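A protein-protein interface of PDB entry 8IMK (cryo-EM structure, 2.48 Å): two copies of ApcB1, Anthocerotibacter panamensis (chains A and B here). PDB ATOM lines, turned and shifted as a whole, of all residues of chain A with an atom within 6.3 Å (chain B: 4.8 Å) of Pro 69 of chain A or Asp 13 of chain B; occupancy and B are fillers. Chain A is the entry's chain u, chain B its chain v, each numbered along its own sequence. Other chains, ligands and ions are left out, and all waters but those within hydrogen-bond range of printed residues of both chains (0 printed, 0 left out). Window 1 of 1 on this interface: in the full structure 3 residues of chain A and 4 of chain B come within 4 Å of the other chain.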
ATOM      1  N   ASP A  65      -9.606  15.379  27.105  1.00  0.00           N
ATOM      2  CA  ASP A  65     -10.478  15.849  26.036  1.00  0.00           C
ATOM      3  C   ASP A  65      -9.684  16.229  24.794  1.00  0.00           C
ATOM      4  O   ASP A  65     -10.223  16.237  23.682  1.00  0.00           O
ATOM      5  CB  ASP A  65     -11.299  17.039  26.525  1.00  0.00           C
ATOM      6  CG  ASP A  65     -10.453  18.068  27.251  1.00  0.00           C
ATOM      7  OD1 ASP A  65      -9.747  17.687  28.209  1.00  0.00           O
ATOM      8  OD2 ASP A  65     -10.491  19.253  26.861  1.00  0.00           O
ATOM      9  N   LEU A  67      -7.479  14.618  23.284  1.00  0.00           N
ATOM     10  CA  LEU A  67      -7.214  13.489  22.404  1.00  0.00           C
ATOM     11  C   LEU A  67      -8.493  12.911  21.820  1.00  0.00           C
ATOM     12  O   LEU A  67      -8.443  12.208  20.806  1.00  0.00           O
ATOM     13  CB  LEU A  67      -6.458  12.407  23.163  1.00  0.00           C
ATOM     14  CG  LEU A  67      -5.089  12.764  23.723  1.00  0.00           C
ATOM     15  CD1 LEU A  67      -4.526  11.569  24.450  1.00  0.00           C
ATOM     16  CD2 LEU A  67      -4.149  13.228  22.631  1.00  0.00           C
ATOM     17  N   ARG A  68      -9.635  13.177  22.445  1.00  0.00           N
ATOM     18  CA  ARG A  68     -10.896  12.644  21.970  1.00  0.00           C
ATOM     19  C   ARG A  68     -11.266  13.259  20.624  1.00  0.00           C
ATOM     20  O   ARG A  68     -10.873  14.385  20.316  1.00  0.00           O
ATOM     21  CB  ARG A  68     -12.003  12.903  22.986  1.00  0.00           C
ATOM     22  CG  ARG A  68     -11.978  11.970  24.175  1.00  0.00           C
ATOM     23  CD  ARG A  68     -13.267  12.060  24.971  1.00  0.00           C
ATOM     24  NE  ARG A  68     -13.297  13.216  25.861  1.00  0.00           N
ATOM     25  CZ  ARG A  68     -12.858  13.202  27.116  1.00  0.00           C
ATOM     26  NH1 ARG A  68     -12.355  12.088  27.632  1.00  0.00           N
ATOM     27  NH2 ARG A  68     -12.924  14.300  27.856  1.00  0.00           N
ATOM     28  N   PRO A  69     -12.005  12.524  19.796  1.00  0.00           N
ATOM     29  CA  PRO A  69     -12.389  13.050  18.481  1.00  0.00           C
ATOM     30  C   PRO A  69     -13.144  14.363  18.603  1.00  0.00           C
ATOM     31  O   PRO A  69     -14.116  14.476  19.351  1.00  0.00           O
ATOM     32  CB  PRO A  69     -13.263  11.936  17.907  1.00  0.00           C
ATOM     33  CG  PRO A  69     -12.743  10.709  18.564  1.00  0.00           C
ATOM     34  CD  PRO A  69     -12.417  11.122  19.960  1.00  0.00           C
ATOM     35  N   GLY A  70     -12.694  15.352  17.840  1.00  0.00           N
ATOM     36  CA  GLY A  70     -13.086  16.723  18.049  1.00  0.00           C
ATOM     37  C   GLY A  70     -12.141  17.519  18.920  1.00  0.00           C
ATOM     38  O   GLY A  70     -12.288  18.744  19.003  1.00  0.00           O
ATOM     39  N   GLY A  71     -11.177  16.866  19.573  1.00  0.00           N
ATOM     40  CA  GLY A  71     -10.160  17.585  20.300  1.00  0.00           C
ATOM     41  C   GLY A  71      -9.148  18.225  19.377  1.00  0.00           C
ATOM     42  O   GLY A  71      -9.051  17.894  18.199  1.00  0.00           O
ATOM     43  N   TYR A  74      -6.595  15.661  18.517  1.00  0.00           N
ATOM     44  CA  TYR A  74      -7.095  14.460  17.871  1.00  0.00           C
ATOM     45  C   TYR A  74      -6.807  14.487  16.380  1.00  0.00           C
ATOM     46  O   TYR A  74      -7.536  15.112  15.611  1.00  0.00           O
ATOM     47  CB  TYR A  74      -8.597  14.312  18.085  1.00  0.00           C
ATOM     48  CG  TYR A  74      -9.199  13.219  17.235  1.00  0.00           C
ATOM     49  CD1 TYR A  74      -9.063  11.888  17.589  1.00  0.00           C
ATOM     50  CD2 TYR A  74      -9.888  13.517  16.068  1.00  0.00           C
ATOM     51  CE1 TYR A  74      -9.602  10.892  16.812  1.00  0.00           C
ATOM     52  CE2 TYR A  74     -10.418  12.528  15.284  1.00  0.00           C
ATOM     53  CZ  TYR A  74     -10.278  11.220  15.661  1.00  0.00           C
ATOM     54  OH  TYR A  74     -10.822  10.233  14.876  1.00  0.00           O
ATOM     55  N   THR A  75      -5.656  13.931  16.016  1.00  0.00           N
ATOM     56  CA  THR A  75      -5.291  13.235  14.782  1.00  0.00           C
ATOM     57  C   THR A  75      -3.828  12.882  14.978  1.00  0.00           C
ATOM     58  O   THR A  75      -3.195  13.398  15.901  1.00  0.00           O
ATOM     59  CB  THR A  75      -5.492  14.032  13.476  1.00  0.00           C
ATOM     60  OG1 THR A  75      -4.783  15.280  13.515  1.00  0.00           O
ATOM     61  CG2 THR A  75      -6.951  14.176  13.036  1.00  0.00           C
ATOM     62  N   ARG A  78      -2.248  16.345  14.216  1.00  0.00           N
ATOM     63  CA  ARG A  78      -2.389  17.377  15.234  1.00  0.00           C
ATOM     64  C   ARG A  78      -1.691  16.976  16.527  1.00  0.00           C
ATOM     65  O   ARG A  78      -1.106  17.822  17.209  1.00  0.00           O
ATOM     66  CB  ARG A  78      -3.867  17.685  15.463  1.00  0.00           C
ATOM     67  CG  ARG A  78      -4.381  18.813  14.581  1.00  0.00           C
ATOM     68  CD  ARG A  78      -5.827  19.180  14.874  1.00  0.00           C
ATOM     69  NE  ARG A  78      -6.765  18.493  14.001  1.00  0.00           N
ATOM     70  CZ  ARG A  78      -7.831  17.832  14.425  1.00  0.00           C
ATOM     71  NH1 ARG A  78      -8.102  17.764  15.717  1.00  0.00           N
ATOM     72  NH2 ARG A  78      -8.626  17.235  13.552  1.00  0.00           N
ATOM     73  N   ILE B   9     -17.462  12.077   5.647  1.00  0.00           N
ATOM     74  CA  ILE B   9     -16.347  11.456   6.355  1.00  0.00           C
ATOM     75  C   ILE B   9     -15.860  12.361   7.473  1.00  0.00           C
ATOM     76  O   ILE B   9     -15.596  11.905   8.588  1.00  0.00           O
ATOM     77  CB  ILE B   9     -15.213  11.115   5.373  1.00  0.00           C
ATOM     78  CG1 ILE B   9     -15.640  10.000   4.426  1.00  0.00           C
ATOM     79  CG2 ILE B   9     -13.949  10.727   6.116  1.00  0.00           C
ATOM     80  CD1 ILE B   9     -14.744   9.855   3.240  1.00  0.00           C
ATOM     81  N   ASN B  10     -15.731  13.658   7.193  1.00  0.00           N
ATOM     82  CA  ASN B  10     -15.265  14.597   8.207  1.00  0.00           C
ATOM     83  C   ASN B  10     -16.270  14.736   9.336  1.00  0.00           C
ATOM     84  O   ASN B  10     -15.889  14.854  10.506  1.00  0.00           O
ATOM     85  CB  ASN B  10     -14.991  15.953   7.568  1.00  0.00           C
ATOM     86  CG  ASN B  10     -13.782  15.929   6.675  1.00  0.00           C
ATOM     87  OD1 ASN B  10     -13.004  14.980   6.687  1.00  0.00           O
ATOM     88  ND2 ASN B  10     -13.610  16.982   5.891  1.00  0.00           N
ATOM     89  N   ARG B  11     -17.558  14.739   9.005  1.00  0.00           N
ATOM     90  CA  ARG B  11     -18.587  14.812  10.035  1.00  0.00           C
ATOM     91  C   ARG B  11     -18.533  13.602  10.954  1.00  0.00           C
ATOM     92  O   ARG B  11     -18.648  13.736  12.176  1.00  0.00           O
ATOM     93  CB  ARG B  11     -19.960  14.944   9.384  1.00  0.00           C
ATOM     94  CG  ARG B  11     -21.092  15.133  10.357  1.00  0.00           C
ATOM     95  CD  ARG B  11     -22.407  15.272   9.619  1.00  0.00           C
ATOM     96  NE  ARG B  11     -22.794  14.039   8.939  1.00  0.00           N
ATOM     97  CZ  ARG B  11     -23.809  13.949   8.086  1.00  0.00           C
ATOM     98  NH1 ARG B  11     -24.539  15.020   7.809  1.00  0.00           N
ATOM     99  NH2 ARG B  11     -24.098  12.789   7.511  1.00  0.00           N
ATOM    100  N   THR B  12     -18.357  12.408  10.387  1.00  0.00           N
ATOM    101  CA  THR B  12     -18.215  11.221  11.225  1.00  0.00           C
ATOM    102  C   THR B  12     -16.923  11.264  12.032  1.00  0.00           C
ATOM    103  O   THR B  12     -16.894  10.836  13.189  1.00  0.00           O
ATOM    104  CB  THR B  12     -18.258   9.955  10.372  1.00  0.00           C
ATOM    105  OG1 THR B  12     -17.181   9.979   9.431  1.00  0.00           O
ATOM    106  CG2 THR B  12     -19.567   9.866   9.617  1.00  0.00           C
ATOM    107  N   ASP B  13     -15.845  11.776  11.437  1.00  0.00           N
ATOM    108  CA  ASP B  13     -14.550  11.777  12.107  1.00  0.00           C
ATOM    109  C   ASP B  13     -14.530  12.739  13.286  1.00  0.00           C
ATOM    110  O   ASP B  13     -13.909  12.454  14.315  1.00  0.00           O
ATOM    111  CB  ASP B  13     -13.451  12.129  11.105  1.00  0.00           C
ATOM    112  CG  ASP B  13     -12.081  12.202  11.744  1.00  0.00           C
ATOM    113  OD1 ASP B  13     -11.602  11.170  12.250  1.00  0.00           O
ATOM    114  OD2 ASP B  13     -11.477  13.298  11.730  1.00  0.00           O
ATOM    115  N   ALA B  14     -15.197  13.887  13.156  1.00  0.00           N
ATOM    116  CA  ALA B  14     -15.231  14.846  14.254  1.00  0.00           C
ATOM    117  C   ALA B  14     -15.926  14.258  15.471  1.00  0.00           C
ATOM    118  O   ALA B  14     -15.662  14.667  16.607  1.00  0.00           O
ATOM    119  CB  ALA B  14     -15.923  16.132  13.808  1.00  0.00           C
ATOM    120  N   GLU B  15     -16.818  13.301  15.252  1.00  0.00           N
ATOM    121  CA  GLU B  15     -17.467  12.560  16.322  1.00  0.00           C
ATOM    122  C   GLU B  15     -16.740  11.270  16.660  1.00  0.00           C
ATOM    123  O   GLU B  15     -17.054  10.645  17.676  1.00  0.00           O
ATOM    124  CB  GLU B  15     -18.911  12.257  15.930  1.00  0.00           C
ATOM    125  CG  GLU B  15     -19.774  13.500  15.838  1.00  0.00           C
ATOM    126  CD  GLU B  15     -21.194  13.200  15.429  1.00  0.00           C
ATOM    127  OE1 GLU B  15     -21.484  12.035  15.093  1.00  0.00           O
ATOM    128  OE2 GLU B  15     -22.025  14.131  15.444  1.00  0.00           O
ATOM    129  N   GLY B  16     -15.777  10.865  15.841  1.00  0.00           N
ATOM    130  CA  GLY B  16     -15.041   9.636  16.075  1.00  0.00           C
ATOM    131  C   GLY B  16     -15.889   8.388  16.021  1.00  0.00           C
ATOM    132  O   GLY B  16     -15.686   7.466  16.820  1.00  0.00           O
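The backbone NH (N) of Gly 70 of chain A is in hydrogen-bond range of the backbone carbonyl oxygen (O) of Ala 14 of chain B, at 3.3 Å.
The side-chain carboxylate of Asp 13 of chain B is in hydrogen-bond range of the side-chain hydroxyl of Tyr 74 of chain A (2.9 Å).
The backbone carbonyl oxygen (O) of Pro 69 of chain A lies close to the backbone carbonyl oxygen (O) of Ala 14 of chain B.
Pro 69 of chain A touches just these residues of chain B: Asp 13 (3.7 Å), Ala 14 (3.2 Å), Glu 15 (3.8 Å) and Gly 16 (3.4 Å).
Of the printed residues of chain B, Gly 70 of chain A touches Ala 14 (3.3 Å).
Printed residues of chain B within 4 Å of Tyr 74 of chain A: Asp 13.
Asp 13 of chain B touches just these residues of chain A: Pro 69 and Tyr 74.
Of the printed residues of chain A, Ala 14 of chain B touches Pro 69 and Gly 70.
Printed residues of chain A within 4 Å of Glu 15 of chain B: Pro 69.
Of the printed residues of chain A, Gly 16 of chain B touches Pro 69 (3.4 Å).
The nearest printed residue of chain B that does not touch Pro 69 of chain A is Thr 12 of chain B (6.1 Å).
The nearest printed residue of chain A that does not touch Ala 14 of chain B is Tyr 74 of chain A (5.4 Å).
No position is printed for both chains.
The backbone carbonyl oxygen of Tyr 74 of chain A sits at hydrogen-bond distance from the guanidinium group of Arg 78 of chain A, at 2.7 Å.
Of the 9 printed residues of chain A, 3 touch a printed residue of chain B.
Hydrophobic or aromatic side chains of chain A that line the printed part of chain B: Pro 69 and Tyr 74.
Among the printed residues, 6 pairs touch across the chains.
Among the printed residues, no Asp or Glu carboxylate lies within 4 Å of a Lys or Arg side-chain nitrogen of the other chain.
Among the printed residues, merely in contact across the chains: Pro 69 of chain A with Asp 13 of chain B (3.7 Å), Pro 69 of chain A with Glu 15 of chain B (3.8 Å) and Pro 69 of chain A with Gly 16 of chain B (3.4 Å).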
